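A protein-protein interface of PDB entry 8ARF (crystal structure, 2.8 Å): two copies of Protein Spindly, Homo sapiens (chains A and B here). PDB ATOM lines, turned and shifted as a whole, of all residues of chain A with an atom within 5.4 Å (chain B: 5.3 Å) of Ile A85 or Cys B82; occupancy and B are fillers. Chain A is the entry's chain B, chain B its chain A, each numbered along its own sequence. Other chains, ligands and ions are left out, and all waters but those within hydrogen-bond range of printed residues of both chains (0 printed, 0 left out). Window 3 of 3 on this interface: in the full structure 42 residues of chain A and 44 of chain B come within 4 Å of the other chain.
The side-chain sulfur of Cys A82 is disulfide-bonded to the side-chain sulfur of Cys B82, at 2.2 Å.
NE2 of Gln B89 sits at hydrogen-bond distance from O of Ile A85 (3.5 Å).
OE1 of Glu B81 lies within salt-bridge range of NZ of Lys A86.
The side-chain amide oxygen of Gln A88 sits at hydrogen-bond distance from the side-chain amide nitrogen of Gln B89 (3.0 Å).
O of Leu A78 sits close to SG of Cys B82 (3.7 Å).
The backbone carbonyl oxygen (O) of Leu B78 sits close to the side-chain sulfur (SG) of Cys A82 (3.7 Å).
Among the printed residues, merely in contact across the chains: Leu A78 with Leu B78 (3.2 Å), Leu A78 with Ser B79 (3.8 Å), Ile A85 with Cys B82 (3.8 Å), Ile A85 with Ile B85 (3.3 Å) and Gln A89 with Gln B89 (3.9 Å).
Ile A85 touches three residues of chain B.
Cys B82 touches just these residues of chain A: Leu A78, Cys A82 and Ile A85.
Printed residues of chain B within 4 Å of Leu A78: Leu B78, Ser B79 and Cys B82.
Of the printed residues of chain B, Cys A82 touches Leu B78 and Cys B82.
Printed residues of chain A within 4 Å of Glu B81: Lys A86.
Of the printed residues of chain A, Gln B89 touches Ile A85, Gln A88 and Gln A89.
Ser B77 touches none of the printed residues of chain A.
The nearest residue of chain B that does not touch Ile A85 is Lys B86 (4.8 Å).
Of the 11 printed residues of chain A, 6 touch a printed residue of chain B.
Hydrophobic or aromatic side chains of chain A that line the printed part of chain B: Leu A78 and Ile A85.
Hydrophobic or aromatic side chains of chain B that line the printed part of chain A: Leu B78 and Ile B85.
Among the printed residues, Asp or Glu carboxylates within 4 Å of a Lys or Arg side-chain nitrogen of the other chain: Lys A86 with Glu B81 (3.6 Å).
Leu B78 touches its own counterpart, Leu A78.
Ile A85 touches Cys B82, but with the chains exchanged Cys A82 does not touch Ile B85 (5.4 Å).
Ile A85 touches Gln B89, but with the chains exchanged Gln A89 does not touch Ile B85 (4.1 Å).
Lys A86 touches Glu B81, but with the chains exchanged Glu A81 does not touch Lys B86 (7.0 Å).
9 positions are printed for both chains.
Of the 11 pairs that touch across the chains among the printed residues, 6 have their exchanged pair printed and touching as well.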
ATOM      1  N   LEU A  78      -3.976 -10.734  11.996  1.00  0.00           N
ATOM      2  CA  LEU A  78      -3.023 -11.735  11.630  1.00  0.00           C
ATOM      3  C   LEU A  78      -3.566 -13.122  11.967  1.00  0.00           C
ATOM      4  O   LEU A  78      -3.316 -14.090  11.237  1.00  0.00           O
ATOM      5  CB  LEU A  78      -1.737 -11.494  12.434  1.00  0.00           C
ATOM      6  CG  LEU A  78      -0.423 -11.388  11.716  1.00  0.00           C
ATOM      7  CD1 LEU A  78      -0.511 -10.106  10.896  1.00  0.00           C
ATOM      8  CD2 LEU A  78       0.716 -11.352  12.715  1.00  0.00           C
ATOM      9  N   CYS A  80      -6.599 -14.071  12.138  1.00  0.00           N
ATOM     10  CA  CYS A  80      -7.664 -14.385  11.230  1.00  0.00           C
ATOM     11  C   CYS A  80      -7.065 -14.782   9.834  1.00  0.00           C
ATOM     12  O   CYS A  80      -7.621 -15.589   9.122  1.00  0.00           O
ATOM     13  CB  CYS A  80      -8.639 -13.215  11.186  1.00  0.00           C
ATOM     14  SG  CYS A  80      -8.498 -12.093   9.758  1.00  0.00           S
ATOM     15  N   GLU A  81      -5.939 -14.187   9.451  1.00  0.00           N
ATOM     16  CA  GLU A  81      -5.225 -14.549   8.216  1.00  0.00           C
ATOM     17  C   GLU A  81      -4.659 -15.962   8.309  1.00  0.00           C
ATOM     18  O   GLU A  81      -5.027 -16.833   7.577  1.00  0.00           O
ATOM     19  CB  GLU A  81      -4.068 -13.575   7.925  1.00  0.00           C
ATOM     20  CG  GLU A  81      -3.272 -13.808   6.644  1.00  0.00           C
ATOM     21  CD  GLU A  81      -3.788 -12.956   5.457  1.00  0.00           C
ATOM     22  OE1 GLU A  81      -3.222 -11.864   5.192  1.00  0.00           O
ATOM     23  OE2 GLU A  81      -4.774 -13.350   4.773  1.00  0.00           O
ATOM     24  N   CYS A  82      -3.785 -16.197   9.269  1.00  0.00           N
ATOM     25  CA  CYS A  82      -3.174 -17.529   9.458  1.00  0.00           C
ATOM     26  C   CYS A  82      -4.197 -18.641   9.375  1.00  0.00           C
ATOM     27  O   CYS A  82      -4.031 -19.599   8.664  1.00  0.00           O
ATOM     28  CB  CYS A  82      -2.466 -17.675  10.816  1.00  0.00           C
ATOM     29  SG  CYS A  82      -0.717 -17.362  10.677  1.00  0.00           S
ATOM     30  N   GLU A  83      -5.295 -18.494  10.109  1.00  0.00           N
ATOM     31  CA  GLU A  83      -6.347 -19.477  10.135  1.00  0.00           C
ATOM     32  C   GLU A  83      -6.900 -19.704   8.703  1.00  0.00           C
ATOM     33  O   GLU A  83      -7.102 -20.833   8.273  1.00  0.00           O
ATOM     34  CB  GLU A  83      -7.434 -19.033  11.122  1.00  0.00           C
ATOM     35  CG  GLU A  83      -8.796 -19.675  10.872  1.00  0.00           C
ATOM     36  CD  GLU A  83      -9.908 -18.662  10.628  1.00  0.00           C
ATOM     37  OE1 GLU A  83      -9.828 -17.911   9.612  1.00  0.00           O
ATOM     38  OE2 GLU A  83     -10.861 -18.647  11.451  1.00  0.00           O
ATOM     39  N   ALA A  84      -7.186 -18.612   7.999  1.00  0.00           N
ATOM     40  CA  ALA A  84      -7.714 -18.678   6.656  1.00  0.00           C
ATOM     41  C   ALA A  84      -6.758 -19.383   5.691  1.00  0.00           C
ATOM     42  O   ALA A  84      -7.132 -20.284   4.943  1.00  0.00           O
ATOM     43  CB  ALA A  84      -8.046 -17.290   6.150  1.00  0.00           C
ATOM     44  N   ILE A  85      -5.504 -18.959   5.715  1.00  0.00           N
ATOM     45  CA  ILE A  85      -4.517 -19.528   4.813  1.00  0.00           C
ATOM     46  C   ILE A  85      -4.092 -20.951   5.224  1.00  0.00           C
ATOM     47  O   ILE A  85      -3.568 -21.713   4.421  1.00  0.00           O
ATOM     48  CB  ILE A  85      -3.312 -18.583   4.606  1.00  0.00           C
ATOM     49  CG1 ILE A  85      -2.638 -18.226   5.925  1.00  0.00           C
ATOM     50  CG2 ILE A  85      -3.806 -17.318   3.875  1.00  0.00           C
ATOM     51  CD1 ILE A  85      -1.642 -17.089   5.769  1.00  0.00           C
ATOM     52  N   LYS A  86      -4.418 -21.350   6.449  1.00  0.00           N
ATOM     53  CA  LYS A  86      -4.278 -22.745   6.870  1.00  0.00           C
ATOM     54  C   LYS A  86      -5.462 -23.557   6.373  1.00  0.00           C
ATOM     55  O   LYS A  86      -5.302 -24.701   6.006  1.00  0.00           O
ATOM     56  CB  LYS A  86      -4.177 -22.877   8.392  1.00  0.00           C
ATOM     57  CG  LYS A  86      -2.775 -23.157   8.894  1.00  0.00           C
ATOM     58  CD  LYS A  86      -2.831 -23.494  10.361  1.00  0.00           C
ATOM     59  CE  LYS A  86      -3.303 -22.254  11.104  1.00  0.00           C
ATOM     60  NZ  LYS A  86      -2.642 -22.173  12.422  1.00  0.00           N
ATOM     61  N   GLN A  87      -6.645 -22.946   6.345  1.00  0.00           N
ATOM     62  CA  GLN A  87      -7.829 -23.613   5.837  1.00  0.00           C
ATOM     63  C   GLN A  87      -7.677 -23.844   4.339  1.00  0.00           C
ATOM     64  O   GLN A  87      -8.195 -24.829   3.791  1.00  0.00           O
ATOM     65  CB  GLN A  87      -9.093 -22.775   6.102  1.00  0.00           C
ATOM     66  CG  GLN A  87     -10.226 -23.550   6.729  1.00  0.00           C
ATOM     67  CD  GLN A  87     -10.963 -24.433   5.720  1.00  0.00           C
ATOM     68  OE1 GLN A  87     -11.476 -23.939   4.701  1.00  0.00           O
ATOM     69  NE2 GLN A  87     -11.020 -25.751   5.994  1.00  0.00           N
ATOM     70  N   GLN A  88      -7.033 -22.898   3.668  1.00  0.00           N
ATOM     71  CA  GLN A  88      -6.760 -23.068   2.259  1.00  0.00           C
ATOM     72  C   GLN A  88      -5.989 -24.347   2.034  1.00  0.00           C
ATOM     73  O   GLN A  88      -6.339 -25.163   1.152  1.00  0.00           O
ATOM     74  CB  GLN A  88      -5.986 -21.871   1.731  1.00  0.00           C
ATOM     75  CG  GLN A  88      -6.917 -20.674   1.467  1.00  0.00           C
ATOM     76  CD  GLN A  88      -6.145 -19.415   1.342  1.00  0.00           C
ATOM     77  OE1 GLN A  88      -4.987 -19.433   0.942  1.00  0.00           O
ATOM     78  NE2 GLN A  88      -6.752 -18.328   1.707  1.00  0.00           N
ATOM     79  N   GLN A  89      -4.935 -24.507   2.831  1.00  0.00           N
ATOM     80  CA  GLN A  89      -4.117 -25.689   2.742  1.00  0.00           C
ATOM     81  C   GLN A  89      -4.915 -26.958   3.099  1.00  0.00           C
ATOM     82  O   GLN A  89      -4.689 -28.036   2.513  1.00  0.00           O
ATOM     83  CB  GLN A  89      -2.931 -25.570   3.670  1.00  0.00           C
ATOM     84  CG  GLN A  89      -1.954 -24.503   3.253  1.00  0.00           C
ATOM     85  CD  GLN A  89      -0.718 -24.567   4.093  1.00  0.00           C
ATOM     86  OE1 GLN A  89       0.419 -24.672   3.583  1.00  0.00           O
ATOM     87  NE2 GLN A  89      -0.926 -24.570   5.404  1.00  0.00           N
ATOM     88  N   SER B  77       5.550 -14.437  16.393  1.00  0.00           N
ATOM     89  CA  SER B  77       5.426 -15.824  16.087  1.00  0.00           C
ATOM     90  C   SER B  77       4.606 -16.024  14.820  1.00  0.00           C
ATOM     91  O   SER B  77       5.083 -16.588  13.849  1.00  0.00           O
ATOM     92  CB  SER B  77       4.818 -16.572  17.269  1.00  0.00           C
ATOM     93  OG  SER B  77       4.021 -17.633  16.804  1.00  0.00           O
ATOM     94  N   LEU B  78       3.345 -15.619  14.822  1.00  0.00           N
ATOM     95  CA  LEU B  78       2.525 -15.926  13.687  1.00  0.00           C
ATOM     96  C   LEU B  78       2.538 -14.806  12.673  1.00  0.00           C
ATOM     97  O   LEU B  78       1.729 -14.763  11.819  1.00  0.00           O
ATOM     98  CB  LEU B  78       1.116 -16.315  14.154  1.00  0.00           C
ATOM     99  CG  LEU B  78       0.296 -15.369  15.011  1.00  0.00           C
ATOM    100  CD1 LEU B  78       0.006 -14.085  14.305  1.00  0.00           C
ATOM    101  CD2 LEU B  78      -1.008 -16.048  15.357  1.00  0.00           C
ATOM    102  N   SER B  79       3.497 -13.887  12.790  1.00  0.00           N
ATOM    103  CA  SER B  79       3.965 -13.134  11.650  1.00  0.00           C
ATOM    104  C   SER B  79       4.829 -14.099  10.849  1.00  0.00           C
ATOM    105  O   SER B  79       4.725 -14.200   9.659  1.00  0.00           O
ATOM    106  CB  SER B  79       4.783 -11.925  12.086  1.00  0.00           C
ATOM    107  OG  SER B  79       5.540 -11.468  10.954  1.00  0.00           O
ATOM    108  N   CYS B  80       5.665 -14.861  11.542  1.00  0.00           N
ATOM    109  CA  CYS B  80       6.473 -15.889  10.913  1.00  0.00           C
ATOM    110  C   CYS B  80       5.581 -16.896  10.272  1.00  0.00           C
ATOM    111  O   CYS B  80       5.533 -16.904   9.031  1.00  0.00           O
ATOM    112  CB  CYS B  80       7.478 -16.499  11.882  1.00  0.00           C
ATOM    113  SG  CYS B  80       8.704 -15.193  12.262  1.00  0.00           S
ATOM    114  N   GLU B  81       4.840 -17.678  11.082  1.00  0.00           N
ATOM    115  CA  GLU B  81       3.970 -18.724  10.539  1.00  0.00           C
ATOM    116  C   GLU B  81       3.261 -18.222   9.246  1.00  0.00           C
ATOM    117  O   GLU B  81       3.350 -18.809   8.190  1.00  0.00           O
ATOM    118  CB  GLU B  81       2.952 -19.174  11.557  1.00  0.00           C
ATOM    119  CG  GLU B  81       2.725 -20.657  11.566  1.00  0.00           C
ATOM    120  CD  GLU B  81       1.277 -21.099  11.881  1.00  0.00           C
ATOM    121  OE1 GLU B  81       0.732 -21.867  11.071  1.00  0.00           O
ATOM    122  OE2 GLU B  81       0.675 -20.738  12.918  1.00  0.00           O
ATOM    123  N   CYS B  82       2.586 -17.084   9.334  1.00  0.00           N
ATOM    124  CA  CYS B  82       1.800 -16.588   8.226  1.00  0.00           C
ATOM    125  C   CYS B  82       2.592 -16.362   7.006  1.00  0.00           C
ATOM    126  O   CYS B  82       2.100 -16.487   5.914  1.00  0.00           O
ATOM    127  CB  CYS B  82       1.087 -15.309   8.614  1.00  0.00           C
ATOM    128  SG  CYS B  82      -0.599 -15.616   9.321  1.00  0.00           S
ATOM    129  N   GLU B  83       3.855 -15.992   7.175  1.00  0.00           N
ATOM    130  CA  GLU B  83       4.724 -15.643   6.031  1.00  0.00           C
ATOM    131  C   GLU B  83       5.327 -16.938   5.431  1.00  0.00           C
ATOM    132  O   GLU B  83       5.496 -17.001   4.206  1.00  0.00           O
ATOM    133  CB  GLU B  83       5.710 -14.511   6.439  1.00  0.00           C
ATOM    134  CG  GLU B  83       7.143 -14.621   5.973  1.00  0.00           C
ATOM    135  CD  GLU B  83       8.077 -15.136   7.065  1.00  0.00           C
ATOM    136  OE1 GLU B  83       8.865 -14.277   7.554  1.00  0.00           O
ATOM    137  OE2 GLU B  83       8.007 -16.377   7.430  1.00  0.00           O
ATOM    138  N   ALA B  84       5.572 -17.952   6.292  1.00  0.00           N
ATOM    139  CA  ALA B  84       5.974 -19.318   5.905  1.00  0.00           C
ATOM    140  C   ALA B  84       4.887 -19.933   5.036  1.00  0.00           C
ATOM    141  O   ALA B  84       5.066 -20.125   3.844  1.00  0.00           O
ATOM    142  CB  ALA B  84       6.214 -20.213   7.105  1.00  0.00           C
ATOM    143  N   ILE B  85       3.707 -20.163   5.603  1.00  0.00           N
ATOM    144  CA  ILE B  85       2.669 -20.882   4.883  1.00  0.00           C
ATOM    145  C   ILE B  85       2.377 -20.196   3.562  1.00  0.00           C
ATOM    146  O   ILE B  85       2.113 -20.852   2.571  1.00  0.00           O
ATOM    147  CB  ILE B  85       1.391 -21.185   5.728  1.00  0.00           C
ATOM    148  CG1 ILE B  85       0.301 -20.127   5.555  1.00  0.00           C
ATOM    149  CG2 ILE B  85       1.709 -21.386   7.204  1.00  0.00           C
ATOM    150  CD1 ILE B  85      -0.437 -20.211   4.227  1.00  0.00           C
ATOM    151  N   LYS B  86       2.414 -18.868   3.532  1.00  0.00           N
ATOM    152  CA  LYS B  86       2.093 -18.160   2.310  1.00  0.00           C
ATOM    153  C   LYS B  86       3.153 -18.520   1.240  1.00  0.00           C
ATOM    154  O   LYS B  86       2.806 -18.466   0.031  1.00  0.00           O
ATOM    155  CB  LYS B  86       1.882 -16.658   2.547  1.00  0.00           C
ATOM    156  CG  LYS B  86       3.143 -15.815   2.532  1.00  0.00           C
ATOM    157  CD  LYS B  86       2.970 -14.392   3.065  1.00  0.00           C
ATOM    158  CE  LYS B  86       3.712 -13.323   2.228  1.00  0.00           C
ATOM    159  NZ  LYS B  86       5.166 -13.462   2.476  1.00  0.00           N
ATOM    160  N   GLN B  89       2.427 -22.073  -0.302  1.00  0.00           N
ATOM    161  CA  GLN B  89       1.425 -21.957  -1.350  1.00  0.00           C
ATOM    162  C   GLN B  89       2.109 -21.530  -2.634  1.00  0.00           C
ATOM    163  O   GLN B  89       1.980 -22.196  -3.653  1.00  0.00           O
ATOM    164  CB  GLN B  89       0.343 -20.942  -0.986  1.00  0.00           C
ATOM    165  CG  GLN B  89      -0.317 -21.170   0.372  1.00  0.00           C
ATOM    166  CD  GLN B  89      -1.723 -20.591   0.448  1.00  0.00           C
ATOM    167  OE1 GLN B  89      -1.994 -19.529  -0.102  1.00  0.00           O
ATOM    168  NE2 GLN B  89      -2.622 -21.294   1.129  1.00  0.00           N
